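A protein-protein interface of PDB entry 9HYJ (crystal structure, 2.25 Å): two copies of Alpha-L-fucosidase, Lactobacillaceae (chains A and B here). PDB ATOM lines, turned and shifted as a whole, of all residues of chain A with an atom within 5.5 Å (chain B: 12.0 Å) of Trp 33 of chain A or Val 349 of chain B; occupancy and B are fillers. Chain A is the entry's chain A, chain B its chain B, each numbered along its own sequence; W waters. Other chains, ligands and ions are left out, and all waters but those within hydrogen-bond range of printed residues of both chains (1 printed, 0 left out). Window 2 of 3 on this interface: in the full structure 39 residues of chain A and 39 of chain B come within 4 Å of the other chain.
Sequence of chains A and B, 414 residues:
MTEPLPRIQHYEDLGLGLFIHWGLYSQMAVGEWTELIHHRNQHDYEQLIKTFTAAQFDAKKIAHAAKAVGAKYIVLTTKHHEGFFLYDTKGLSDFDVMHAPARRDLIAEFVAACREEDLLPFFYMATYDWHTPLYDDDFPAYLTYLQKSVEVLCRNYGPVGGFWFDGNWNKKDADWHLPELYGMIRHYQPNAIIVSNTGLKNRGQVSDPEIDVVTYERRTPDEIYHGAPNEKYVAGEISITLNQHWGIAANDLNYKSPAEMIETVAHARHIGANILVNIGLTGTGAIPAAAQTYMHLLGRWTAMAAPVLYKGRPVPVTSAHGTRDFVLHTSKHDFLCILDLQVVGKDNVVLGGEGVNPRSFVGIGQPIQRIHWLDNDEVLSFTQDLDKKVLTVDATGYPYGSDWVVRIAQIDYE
The backbone NH of Glu 32 of chain A is in hydrogen-bond range of the side-chain hydroxyl of Tyr 400 of chain B (3.2 Å).
The backbone NH of Trp 33 of chain A sits at hydrogen-bond distance from the side-chain hydroxyl of Tyr 400 of chain B (2.9 Å).
O of Tyr 400 of chain B lies within hydrogen-bond range of NE2 of His 38 of chain A (2.9 Å).
The indole nitrogen (NE1) of Trp 169 of chain A is in hydrogen-bond range of the backbone carbonyl oxygen (O) of Asn 348 of chain B, at 3.3 Å.
The side-chain hydroxyl (OG1) of Thr 34 of chain A lies within hydrogen-bond range of a ring nitrogen (ND1) of His 38 of chain A (2.6 Å).
Among the printed residues, merely in contact across the chains: Gly 31 of chain A with Tyr 400 of chain B (3.5 Å), Trp 33 of chain A with Val 349 of chain B (3.8 Å), Thr 34 of chain A with Tyr 400 of chain B (3.8 Å), Ile 37 of chain A with Tyr 400 of chain B (3.4 Å) and Trp 169 of chain A with Val 349 of chain B (3.6 Å).
No residue of chain B comes within 4 Å of Tyr 25 of chain A.
Of chain B, only Tyr 400 (3.5 Å) comes within 4 Å of Gly 31 of chain A.
Of chain B, only Tyr 400 comes within 4 Å of Glu 32 of chain A.
Printed residues of chain B within 4 Å of Trp 33 of chain A: Val 349 (3.8 Å) and Tyr 400 (2.9 Å).
Of chain B, only Tyr 400 (3.8 Å) comes within 4 Å of Thr 34 of chain A.
Of chain B, only Tyr 400 (3.4 Å) comes within 4 Å of Ile 37 of chain A.
Of chain B, only Tyr 400 (2.9 Å) comes within 4 Å of His 38 of chain A.
No residue of chain B comes within 4 Å of Asn 168 of chain A.
Trp 169 of chain A touches just these residues of chain B: Asn 348 (3.3 Å) and Val 349 (3.6 Å).
Printed residues of chain A within 4 Å of Asn 348 of chain B: Trp 169.
Of the printed residues of chain A, Tyr 400 of chain B touches Gly 31, Glu 32, Trp 33, Thr 34, Ile 37 and His 38.
The nearest residue of chain B that does not touch Trp 33 of chain A is Leu 351 of chain B (6.8 Å).
The nearest printed residue of chain A that does not touch Tyr 400 of chain B is Glu 35 of chain A (6.4 Å).
Of the 15 printed residues of chain A, 7 touch a printed residue of chain B.
Hydrophobic or aromatic side chains of chain A that line the printed part of chain B: Trp 33, Ile 37, His 38 and Trp 169.
Along chain A the printed residues that touch a printed residue of chain B span positions 31 to 169.
Of the 20 printed residues of chain B, 3 touch a printed residue of chain A.
Printed residues of chain B that touch a printed residue of chain A: Asn 348, Val 349 and Tyr 400.
Among the printed residues, 9 pairs touch across the chains.
No position is printed for both chains.
Of the 9 pairs that touch across the chains among the printed residues, none has its exchanged pair printed and touching as well.
Water W1 bridges OE2 of Glu 32 of chain A (2.4 Å) and OH of Tyr 400 of chain B (2.6 Å).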
ATOM      1  N   TYR A  25     -30.117 -22.514   5.086  1.00  0.00           N
ATOM      2  CA  TYR A  25     -29.291 -23.712   5.074  1.00  0.00           C
ATOM      3  C   TYR A  25     -28.755 -24.043   6.465  1.00  0.00           C
ATOM      4  O   TYR A  25     -28.548 -25.207   6.779  1.00  0.00           O
ATOM      5  CB  TYR A  25     -28.116 -23.579   4.121  1.00  0.00           C
ATOM      6  CG  TYR A  25     -27.402 -22.244   4.251  1.00  0.00           C
ATOM      7  CD1 TYR A  25     -26.440 -22.020   5.241  1.00  0.00           C
ATOM      8  CD2 TYR A  25     -27.680 -21.210   3.350  1.00  0.00           C
ATOM      9  CE1 TYR A  25     -25.799 -20.785   5.350  1.00  0.00           C
ATOM     10  CE2 TYR A  25     -27.039 -19.980   3.439  1.00  0.00           C
ATOM     11  CZ  TYR A  25     -26.093 -19.772   4.438  1.00  0.00           C
ATOM     12  OH  TYR A  25     -25.488 -18.553   4.510  1.00  0.00           O
ATOM     13  N   GLY A  31     -23.987 -27.694   5.208  1.00  0.00           N
ATOM     14  CA  GLY A  31     -23.319 -26.851   4.204  1.00  0.00           C
ATOM     15  C   GLY A  31     -24.298 -25.888   3.513  1.00  0.00           C
ATOM     16  O   GLY A  31     -25.510 -26.163   3.409  1.00  0.00           O
ATOM     17  N   GLU A  32     -23.776 -24.744   3.063  1.00  0.00           N
ATOM     18  CA  GLU A  32     -24.592 -23.667   2.519  1.00  0.00           C
ATOM     19  C   GLU A  32     -25.113 -24.007   1.115  1.00  0.00           C
ATOM     20  O   GLU A  32     -26.083 -23.410   0.646  1.00  0.00           O
ATOM     21  CB  GLU A  32     -23.915 -22.289   2.566  1.00  0.00           C
ATOM     22  CG  GLU A  32     -22.705 -22.137   1.647  1.00  0.00           C
ATOM     23  CD  GLU A  32     -21.444 -22.974   1.960  1.00  0.00           C
ATOM     24  OE1 GLU A  32     -21.352 -23.702   2.985  1.00  0.00           O
ATOM     25  OE2 GLU A  32     -20.500 -22.872   1.151  1.00  0.00           O
ATOM     26  N   TRP A  33     -24.500 -24.972   0.421  1.00  0.00           N
ATOM     27  CA  TRP A  33     -24.962 -25.300  -0.910  1.00  0.00           C
ATOM     28  C   TRP A  33     -25.970 -26.449  -0.909  1.00  0.00           C
ATOM     29  O   TRP A  33     -26.234 -27.005  -1.972  1.00  0.00           O
ATOM     30  CB  TRP A  33     -23.797 -25.691  -1.817  1.00  0.00           C
ATOM     31  CG  TRP A  33     -23.016 -24.547  -2.398  1.00  0.00           C
ATOM     32  CD1 TRP A  33     -22.202 -23.684  -1.723  1.00  0.00           C
ATOM     33  CD2 TRP A  33     -22.888 -24.220  -3.801  1.00  0.00           C
ATOM     34  NE1 TRP A  33     -21.640 -22.790  -2.591  1.00  0.00           N
ATOM     35  CE2 TRP A  33     -22.011 -23.110  -3.876  1.00  0.00           C
ATOM     36  CE3 TRP A  33     -23.417 -24.751  -4.987  1.00  0.00           C
ATOM     37  CZ2 TRP A  33     -21.657 -22.530  -5.095  1.00  0.00           C
ATOM     38  CZ3 TRP A  33     -23.056 -24.184  -6.197  1.00  0.00           C
ATOM     39  CH2 TRP A  33     -22.177 -23.092  -6.247  1.00  0.00           C
ATOM     40  N   THR A  34     -26.559 -26.780   0.250  1.00  0.00           N
ATOM     41  CA  THR A  34     -27.294 -28.035   0.398  1.00  0.00           C
ATOM     42  C   THR A  34     -28.453 -28.150  -0.612  1.00  0.00           C
ATOM     43  O   THR A  34     -28.691 -29.215  -1.187  1.00  0.00           O
ATOM     44  CB  THR A  34     -27.727 -28.209   1.852  1.00  0.00           C
ATOM     45  OG1 THR A  34     -28.445 -29.419   1.821  1.00  0.00           O
ATOM     46  CG2 THR A  34     -28.706 -27.181   2.384  1.00  0.00           C
ATOM     47  N   GLU A  35     -29.160 -27.067  -0.883  1.00  0.00           N
ATOM     48  CA  GLU A  35     -30.296 -27.151  -1.761  1.00  0.00           C
ATOM     49  C   GLU A  35     -29.953 -27.639  -3.143  1.00  0.00           C
ATOM     50  O   GLU A  35     -30.625 -28.489  -3.645  1.00  0.00           O
ATOM     51  CB  GLU A  35     -31.026 -25.819  -1.835  1.00  0.00           C
ATOM     52  CG  GLU A  35     -32.409 -25.897  -2.454  1.00  0.00           C
ATOM     53  CD  GLU A  35     -33.075 -24.548  -2.680  1.00  0.00           C
ATOM     54  OE1 GLU A  35     -32.425 -23.503  -2.597  1.00  0.00           O
ATOM     55  OE2 GLU A  35     -34.264 -24.545  -2.958  1.00  0.00           O
ATOM     56  N   LEU A  36     -28.929 -27.087  -3.754  1.00  0.00           N
ATOM     57  CA  LEU A  36     -28.494 -27.567  -5.024  1.00  0.00           C
ATOM     58  C   LEU A  36     -27.756 -28.895  -4.986  1.00  0.00           C
ATOM     59  O   LEU A  36     -28.096 -29.799  -5.679  1.00  0.00           O
ATOM     60  CB  LEU A  36     -27.656 -26.510  -5.709  1.00  0.00           C
ATOM     61  CG  LEU A  36     -26.975 -26.880  -7.011  1.00  0.00           C
ATOM     62  CD1 LEU A  36     -28.018 -27.065  -8.061  1.00  0.00           C
ATOM     63  CD2 LEU A  36     -26.062 -25.798  -7.464  1.00  0.00           C
ATOM     64  N   ILE A  37     -26.801 -29.022  -4.089  1.00  0.00           N
ATOM     65  CA  ILE A  37     -25.975 -30.211  -4.014  1.00  0.00           C
ATOM     66  C   ILE A  37     -26.667 -31.504  -3.630  1.00  0.00           C
ATOM     67  O   ILE A  37     -26.394 -32.514  -4.173  1.00  0.00           O
ATOM     68  CB  ILE A  37     -24.634 -29.943  -3.323  1.00  0.00           C
ATOM     69  CG1 ILE A  37     -23.891 -28.894  -4.130  1.00  0.00           C
ATOM     70  CG2 ILE A  37     -23.782 -31.175  -3.274  1.00  0.00           C
ATOM     71  CD1 ILE A  37     -22.650 -28.357  -3.490  1.00  0.00           C
ATOM     72  N   HIS A  38     -27.606 -31.416  -2.723  1.00  0.00           N
ATOM     73  CA  HIS A  38     -28.370 -32.542  -2.259  1.00  0.00           C
ATOM     74  C   HIS A  38     -29.671 -32.731  -3.051  1.00  0.00           C
ATOM     75  O   HIS A  38     -30.512 -33.481  -2.654  1.00  0.00           O
ATOM     76  CB  HIS A  38     -28.647 -32.412  -0.778  1.00  0.00           C
ATOM     77  CG  HIS A  38     -27.429 -32.474   0.064  1.00  0.00           C
ATOM     78  ND1 HIS A  38     -27.162 -31.570   1.050  1.00  0.00           N
ATOM     79  CD2 HIS A  38     -26.393 -33.332   0.058  1.00  0.00           C
ATOM     80  CE1 HIS A  38     -26.016 -31.863   1.614  1.00  0.00           C
ATOM     81  NE2 HIS A  38     -25.534 -32.933   1.034  1.00  0.00           N
ATOM     82  N   HIS A  80     -27.782 -15.528   0.201  1.00  0.00           N
ATOM     83  CA  HIS A  80     -26.891 -16.522  -0.411  1.00  0.00           C
ATOM     84  C   HIS A  80     -27.572 -17.090  -1.667  1.00  0.00           C
ATOM     85  O   HIS A  80     -28.622 -16.594  -2.076  1.00  0.00           O
ATOM     86  CB  HIS A  80     -26.491 -17.551   0.661  1.00  0.00           C
ATOM     87  CG  HIS A  80     -25.140 -18.115   0.419  1.00  0.00           C
ATOM     88  ND1 HIS A  80     -24.888 -19.141  -0.470  1.00  0.00           N
ATOM     89  CD2 HIS A  80     -23.941 -17.749   0.939  1.00  0.00           C
ATOM     90  CE1 HIS A  80     -23.582 -19.385  -0.504  1.00  0.00           C
ATOM     91  NE2 HIS A  80     -22.986 -18.545   0.366  1.00  0.00           N
ATOM     92  N   HIS A  81     -27.000 -18.147  -2.274  1.00  0.00           N
ATOM     93  CA  HIS A  81     -27.549 -18.732  -3.479  1.00  0.00           C
ATOM     94  C   HIS A  81     -29.000 -19.169  -3.264  1.00  0.00           C
ATOM     95  O   HIS A  81     -29.818 -19.078  -4.180  1.00  0.00           O
ATOM     96  CB  HIS A  81     -26.718 -19.939  -3.929  1.00  0.00           C
ATOM     97  CG  HIS A  81     -25.298 -19.610  -4.188  1.00  0.00           C
ATOM     98  ND1 HIS A  81     -24.915 -18.597  -5.032  1.00  0.00           N
ATOM     99  CD2 HIS A  81     -24.161 -20.148  -3.716  1.00  0.00           C
ATOM    100  CE1 HIS A  81     -23.586 -18.524  -5.069  1.00  0.00           C
ATOM    101  NE2 HIS A  81     -23.114 -19.450  -4.272  1.00  0.00           N
ATOM    102  N   TYR A 128     -25.557 -15.578  -8.216  1.00  0.00           N
ATOM    103  CA  TYR A 128     -26.214 -16.769  -8.744  1.00  0.00           C
ATOM    104  C   TYR A 128     -27.308 -17.182  -7.749  1.00  0.00           C
ATOM    105  O   TYR A 128     -27.009 -17.529  -6.604  1.00  0.00           O
ATOM    106  CB  TYR A 128     -25.114 -17.830  -8.814  1.00  0.00           C
ATOM    107  CG  TYR A 128     -25.500 -19.250  -9.196  1.00  0.00           C
ATOM    108  CD1 TYR A 128     -26.610 -19.517 -10.009  1.00  0.00           C
ATOM    109  CD2 TYR A 128     -24.741 -20.334  -8.751  1.00  0.00           C
ATOM    110  CE1 TYR A 128     -26.947 -20.813 -10.373  1.00  0.00           C
ATOM    111  CE2 TYR A 128     -25.050 -21.633  -9.127  1.00  0.00           C
ATOM    112  CZ  TYR A 128     -26.153 -21.867  -9.937  1.00  0.00           C
ATOM    113  OH  TYR A 128     -26.471 -23.143 -10.280  1.00  0.00           O
ATOM    114  N   TRP A 130     -30.900 -19.238  -6.714  1.00  0.00           N
ATOM    115  CA  TRP A 130     -31.666 -20.454  -6.956  1.00  0.00           C
ATOM    116  C   TRP A 130     -33.151 -20.231  -6.670  1.00  0.00           C
ATOM    117  O   TRP A 130     -33.941 -21.140  -6.859  1.00  0.00           O
ATOM    118  CB  TRP A 130     -31.186 -21.621  -6.066  1.00  0.00           C
ATOM    119  CG  TRP A 130     -29.725 -21.953  -6.215  1.00  0.00           C
ATOM    120  CD1 TRP A 130     -28.939 -21.708  -7.310  1.00  0.00           C
ATOM    121  CD2 TRP A 130     -28.865 -22.551  -5.216  1.00  0.00           C
ATOM    122  NE1 TRP A 130     -27.656 -22.143  -7.078  1.00  0.00           N
ATOM    123  CE2 TRP A 130     -27.573 -22.656  -5.800  1.00  0.00           C
ATOM    124  CE3 TRP A 130     -29.050 -22.998  -3.905  1.00  0.00           C
ATOM    125  CZ2 TRP A 130     -26.478 -23.185  -5.109  1.00  0.00           C
ATOM    126  CZ3 TRP A 130     -27.967 -23.508  -3.211  1.00  0.00           C
ATOM    127  CH2 TRP A 130     -26.695 -23.595  -3.805  1.00  0.00           C
ATOM    128  N   ASN A 168     -19.339 -17.022  -8.027  1.00  0.00           N
ATOM    129  CA  ASN A 168     -19.151 -18.440  -8.271  1.00  0.00           C
ATOM    130  C   ASN A 168     -20.337 -19.050  -9.026  1.00  0.00           C
ATOM    131  O   ASN A 168     -21.483 -18.946  -8.567  1.00  0.00           O
ATOM    132  CB  ASN A 168     -19.088 -19.181  -6.939  1.00  0.00           C
ATOM    133  CG  ASN A 168     -17.727 -19.090  -6.290  1.00  0.00           C
ATOM    134  OD1 ASN A 168     -16.723 -18.835  -6.973  1.00  0.00           O
ATOM    135  ND2 ASN A 168     -17.674 -19.328  -4.984  1.00  0.00           N
ATOM    136  N   TRP A 169     -20.029 -19.741 -10.144  1.00  0.00           N
ATOM    137  CA  TRP A 169     -20.981 -20.497 -10.968  1.00  0.00           C
ATOM    138  C   TRP A 169     -22.016 -19.572 -11.650  1.00  0.00           C
ATOM    139  O   TRP A 169     -23.125 -19.969 -12.036  1.00  0.00           O
ATOM    140  CB  TRP A 169     -21.528 -21.772 -10.273  1.00  0.00           C
ATOM    141  CG  TRP A 169     -20.540 -22.919 -10.229  1.00  0.00           C
ATOM    142  CD1 TRP A 169     -20.417 -23.928 -11.141  1.00  0.00           C
ATOM    143  CD2 TRP A 169     -19.500 -23.155  -9.244  1.00  0.00           C
ATOM    144  NE1 TRP A 169     -19.389 -24.765 -10.796  1.00  0.00           N
ATOM    145  CE2 TRP A 169     -18.804 -24.319  -9.639  1.00  0.00           C
ATOM    146  CE3 TRP A 169     -19.075 -22.494  -8.080  1.00  0.00           C
ATOM    147  CZ2 TRP A 169     -17.731 -24.837  -8.906  1.00  0.00           C
ATOM    148  CZ3 TRP A 169     -18.016 -23.009  -7.352  1.00  0.00           C
ATOM    149  CH2 TRP A 169     -17.351 -24.164  -7.765  1.00  0.00           C
ATOM    150  N   GLN B 342     -12.036 -36.771  -0.385  1.00  0.00           N
ATOM    151  CA  GLN B 342     -12.603 -35.439  -0.522  1.00  0.00           C
ATOM    152  C   GLN B 342     -14.128 -35.447  -0.482  1.00  0.00           C
ATOM    153  O   GLN B 342     -14.746 -36.501  -0.567  1.00  0.00           O
ATOM    154  CB  GLN B 342     -11.978 -34.828  -1.772  1.00  0.00           C
ATOM    155  CG  GLN B 342     -10.498 -34.527  -1.523  1.00  0.00           C
ATOM    156  CD  GLN B 342      -9.875 -33.894  -2.736  1.00  0.00           C
ATOM    157  OE1 GLN B 342      -9.568 -34.574  -3.724  1.00  0.00           O
ATOM    158  NE2 GLN B 342      -9.743 -32.575  -2.687  1.00  0.00           N
ATOM    159  N   VAL B 343     -14.713 -34.254  -0.325  1.00  0.00           N
ATOM    160  CA  VAL B 343     -16.143 -34.038  -0.376  1.00  0.00           C
ATOM    161  C   VAL B 343     -16.619 -34.062  -1.829  1.00  0.00           C
ATOM    162  O   VAL B 343     -15.930 -33.610  -2.730  1.00  0.00           O
ATOM    163  CB  VAL B 343     -16.482 -32.709   0.331  1.00  0.00           C
ATOM    164  CG1 VAL B 343     -17.985 -32.453   0.382  1.00  0.00           C
ATOM    165  CG2 VAL B 343     -15.894 -32.656   1.735  1.00  0.00           C
ATOM    166  N   VAL B 344     -17.805 -34.648  -2.050  1.00  0.00           N
ATOM    167  CA  VAL B 344     -18.406 -34.767  -3.373  1.00  0.00           C
ATOM    168  C   VAL B 344     -19.314 -33.564  -3.629  1.00  0.00           C
ATOM    169  O   VAL B 344     -20.218 -33.318  -2.838  1.00  0.00           O
ATOM    170  CB  VAL B 344     -19.214 -36.081  -3.405  1.00  0.00           C
ATOM    171  CG1 VAL B 344     -20.122 -36.202  -4.628  1.00  0.00           C
ATOM    172  CG2 VAL B 344     -18.295 -37.294  -3.334  1.00  0.00           C
ATOM    173  N   GLY B 345     -19.096 -32.858  -4.754  1.00  0.00           N
ATOM    174  CA  GLY B 345     -20.025 -31.869  -5.312  1.00  0.00           C
ATOM    175  C   GLY B 345     -21.116 -32.503  -6.195  1.00  0.00           C
ATOM    176  O   GLY B 345     -21.602 -33.603  -5.914  1.00  0.00           O
ATOM    177  N   LYS B 346     -21.531 -31.816  -7.271  1.00  0.00           N
ATOM    178  CA  LYS B 346     -22.528 -32.386  -8.179  1.00  0.00           C
ATOM    179  C   LYS B 346     -22.388 -31.767  -9.566  1.00  0.00           C
ATOM    180  O   LYS B 346     -22.464 -30.552  -9.690  1.00  0.00           O
ATOM    181  CB  LYS B 346     -23.936 -32.239  -7.594  1.00  0.00           C
ATOM    182  CG  LYS B 346     -25.171 -32.079  -8.491  1.00  0.00           C
ATOM    183  CD  LYS B 346     -25.874 -33.291  -9.092  1.00  0.00           C
ATOM    184  CE  LYS B 346     -27.084 -32.833  -9.865  1.00  0.00           C
ATOM    185  NZ  LYS B 346     -27.927 -33.927 -10.363  1.00  0.00           N
ATOM    186  N   ASP B 347     -22.183 -32.622 -10.576  1.00  0.00           N
ATOM    187  CA  ASP B 347     -22.087 -32.240 -11.983  1.00  0.00           C
ATOM    188  C   ASP B 347     -20.919 -31.282 -12.228  1.00  0.00           C
ATOM    189  O   ASP B 347     -19.764 -31.701 -12.216  1.00  0.00           O
ATOM    190  CB  ASP B 347     -23.412 -31.726 -12.528  1.00  0.00           C
ATOM    191  CG  ASP B 347     -24.570 -32.710 -12.472  1.00  0.00           C
ATOM    192  OD1 ASP B 347     -24.331 -33.918 -12.703  1.00  0.00           O
ATOM    193  OD2 ASP B 347     -25.714 -32.264 -12.252  1.00  0.00           O
ATOM    194  N   ASN B 348     -21.254 -30.000 -12.466  1.00  0.00           N
ATOM    195  CA  ASN B 348     -20.296 -28.947 -12.788  1.00  0.00           C
ATOM    196  C   ASN B 348     -19.616 -28.410 -11.528  1.00  0.00           C
ATOM    197  O   ASN B 348     -18.535 -27.848 -11.638  1.00  0.00           O
ATOM    198  CB  ASN B 348     -20.777 -27.929 -13.826  1.00  0.00           C
ATOM    199  CG  ASN B 348     -21.781 -26.912 -13.326  1.00  0.00           C
ATOM    200  OD1 ASN B 348     -22.565 -27.162 -12.404  1.00  0.00           O
ATOM    201  ND2 ASN B 348     -21.820 -25.762 -13.977  1.00  0.00           N
ATOM    202  N   VAL B 349     -20.243 -28.573 -10.350  1.00  0.00           N
ATOM    203  CA  VAL B 349     -19.681 -28.135  -9.073  1.00  0.00           C
ATOM    204  C   VAL B 349     -18.792 -29.246  -8.495  1.00  0.00           C
ATOM    205  O   VAL B 349     -19.290 -30.213  -7.908  1.00  0.00           O
ATOM    206  CB  VAL B 349     -20.726 -27.592  -8.069  1.00  0.00           C
ATOM    207  CG1 VAL B 349     -20.090 -26.994  -6.808  1.00  0.00           C
ATOM    208  CG2 VAL B 349     -21.682 -26.593  -8.730  1.00  0.00           C
ATOM    209  N   VAL B 350     -17.476 -29.081  -8.707  1.00  0.00           N
ATOM    210  CA  VAL B 350     -16.440 -30.071  -8.441  1.00  0.00           C
ATOM    211  C   VAL B 350     -15.761 -29.713  -7.113  1.00  0.00           C
ATOM    212  O   VAL B 350     -15.105 -28.673  -7.017  1.00  0.00           O
ATOM    213  CB  VAL B 350     -15.436 -30.149  -9.626  1.00  0.00           C
ATOM    214  CG1 VAL B 350     -14.173 -30.971  -9.350  1.00  0.00           C
ATOM    215  CG2 VAL B 350     -16.094 -30.659 -10.898  1.00  0.00           C
ATOM    216  N   LEU B 351     -15.921 -30.589  -6.107  1.00  0.00           N
ATOM    217  CA  LEU B 351     -15.284 -30.394  -4.810  1.00  0.00           C
ATOM    218  C   LEU B 351     -14.090 -31.341  -4.600  1.00  0.00           C
ATOM    219  O   LEU B 351     -13.315 -31.151  -3.660  1.00  0.00           O
ATOM    220  CB  LEU B 351     -16.280 -30.415  -3.645  1.00  0.00           C
ATOM    221  CG  LEU B 351     -17.425 -29.394  -3.698  1.00  0.00           C
ATOM    222  CD1 LEU B 351     -18.355 -29.732  -2.572  1.00  0.00           C
ATOM    223  CD2 LEU B 351     -17.040 -27.918  -3.644  1.00  0.00           C
ATOM    224  N   GLY B 352     -13.936 -32.360  -5.464  1.00  0.00           N
ATOM    225  CA  GLY B 352     -12.738 -33.201  -5.453  1.00  0.00           C
ATOM    226  C   GLY B 352     -12.998 -34.711  -5.394  1.00  0.00           C
ATOM    227  O   GLY B 352     -12.160 -35.491  -5.847  1.00  0.00           O
ATOM    228  N   GLY B 353     -14.155 -35.135  -4.854  1.00  0.00           N
ATOM    229  CA  GLY B 353     -14.364 -36.535  -4.510  1.00  0.00           C
ATOM    230  C   GLY B 353     -15.159 -37.372  -5.519  1.00  0.00           C
ATOM    231  O   GLY B 353     -15.399 -38.546  -5.244  1.00  0.00           O
ATOM    232  N   GLU B 354     -15.545 -36.805  -6.682  1.00  0.00           N
ATOM    233  CA  GLU B 354     -16.642 -37.368  -7.482  1.00  0.00           C
ATOM    234  C   GLU B 354     -16.221 -38.492  -8.449  1.00  0.00           C
ATOM    235  O   GLU B 354     -17.052 -39.327  -8.820  1.00  0.00           O
ATOM    236  CB  GLU B 354     -17.712 -36.377  -7.972  1.00  0.00           C
ATOM    237  CG  GLU B 354     -17.168 -35.082  -8.567  1.00  0.00           C
ATOM    238  CD  GLU B 354     -16.495 -34.074  -7.634  1.00  0.00           C
ATOM    239  OE1 GLU B 354     -15.252 -33.959  -7.742  1.00  0.00           O
ATOM    240  OE2 GLU B 354     -17.170 -33.393  -6.826  1.00  0.00           O
ATOM    241  N   GLY B 355     -14.945 -38.531  -8.858  1.00  0.00           N
ATOM    242  CA  GLY B 355     -14.475 -39.600  -9.729  1.00  0.00           C
ATOM    243  C   GLY B 355     -14.336 -40.917  -8.955  1.00  0.00           C
ATOM    244  O   GLY B 355     -14.244 -40.932  -7.731  1.00  0.00           O
ATOM    245  N   GLY B 397     -16.385 -40.352  -2.156  1.00  0.00           N
ATOM    246  CA  GLY B 397     -16.043 -39.221  -1.328  1.00  0.00           C
ATOM    247  C   GLY B 397     -17.204 -38.890  -0.398  1.00  0.00           C
ATOM    248  O   GLY B 397     -18.260 -39.513  -0.476  1.00  0.00           O
ATOM    249  N   TYR B 398     -16.979 -37.941   0.514  1.00  0.00           N
ATOM    250  CA  TYR B 398     -17.984 -37.619   1.511  1.00  0.00           C
ATOM    251  C   TYR B 398     -19.194 -36.960   0.852  1.00  0.00           C
ATOM    252  O   TYR B 398     -19.057 -36.122  -0.040  1.00  0.00           O
ATOM    253  CB  TYR B 398     -17.429 -36.619   2.527  1.00  0.00           C
ATOM    254  CG  TYR B 398     -16.225 -37.189   3.252  1.00  0.00           C
ATOM    255  CD1 TYR B 398     -16.390 -38.252   4.131  1.00  0.00           C
ATOM    256  CD2 TYR B 398     -14.935 -36.672   3.051  1.00  0.00           C
ATOM    257  CE1 TYR B 398     -15.296 -38.804   4.781  1.00  0.00           C
ATOM    258  CE2 TYR B 398     -13.832 -37.199   3.716  1.00  0.00           C
ATOM    259  CZ  TYR B 398     -14.031 -38.262   4.580  1.00  0.00           C
ATOM    260  OH  TYR B 398     -13.016 -38.860   5.241  1.00  0.00           O
ATOM    261  N   PRO B 399     -20.411 -37.249   1.342  1.00  0.00           N
ATOM    262  CA  PRO B 399     -21.538 -36.397   1.001  1.00  0.00           C
ATOM    263  C   PRO B 399     -21.241 -34.951   1.391  1.00  0.00           C
ATOM    264  O   PRO B 399     -20.694 -34.693   2.459  1.00  0.00           O
ATOM    265  CB  PRO B 399     -22.747 -36.960   1.767  1.00  0.00           C
ATOM    266  CG  PRO B 399     -22.224 -38.239   2.414  1.00  0.00           C
ATOM    267  CD  PRO B 399     -20.718 -38.313   2.311  1.00  0.00           C
ATOM    268  N   TYR B 400     -21.590 -34.020   0.506  1.00  0.00           N
ATOM    269  CA  TYR B 400     -21.518 -32.604   0.812  1.00  0.00           C
ATOM    270  C   TYR B 400     -22.057 -32.384   2.219  1.00  0.00           C
ATOM    271  O   TYR B 400     -23.049 -33.002   2.622  1.00  0.00           O
ATOM    272  CB  TYR B 400     -22.242 -31.790  -0.275  1.00  0.00           C
ATOM    273  CG  TYR B 400     -22.181 -30.301   0.040  1.00  0.00           C
ATOM    274  CD1 TYR B 400     -21.022 -29.565  -0.213  1.00  0.00           C
ATOM    275  CD2 TYR B 400     -23.262 -29.643   0.622  1.00  0.00           C
ATOM    276  CE1 TYR B 400     -20.946 -28.215   0.073  1.00  0.00           C
ATOM    277  CE2 TYR B 400     -23.187 -28.296   0.946  1.00  0.00           C
ATOM    278  CZ  TYR B 400     -22.018 -27.598   0.693  1.00  0.00           C
ATOM    279  OH  TYR B 400     -21.953 -26.278   0.983  1.00  0.00           O
ATOM    280  N   GLY B 401     -21.358 -31.541   2.985  1.00  0.00           N
ATOM    281  CA  GLY B 401     -21.782 -31.200   4.328  1.00  0.00           C
ATOM    282  C   GLY B 401     -21.155 -32.094   5.391  1.00  0.00           C
ATOM    283  O   GLY B 401     -21.384 -31.892   6.578  1.00  0.00           O
ATOM    284  N   SER B 402     -20.377 -33.103   4.987  1.00  0.00           N
ATOM    285  CA  SER B 402     -19.713 -33.907   5.994  1.00  0.00           C
ATOM    286  C   SER B 402     -18.260 -34.196   5.587  1.00  0.00           C
ATOM    287  O   SER B 402     -17.895 -34.039   4.416  1.00  0.00           O
ATOM    288  CB  SER B 402     -20.529 -35.136   6.278  1.00  0.00           C
ATOM    289  OG  SER B 402     -20.352 -36.074   5.215  1.00  0.00           O
HETATM  290  O   HOH W   1     -19.617 -25.143   1.177  1.00  0.00           O
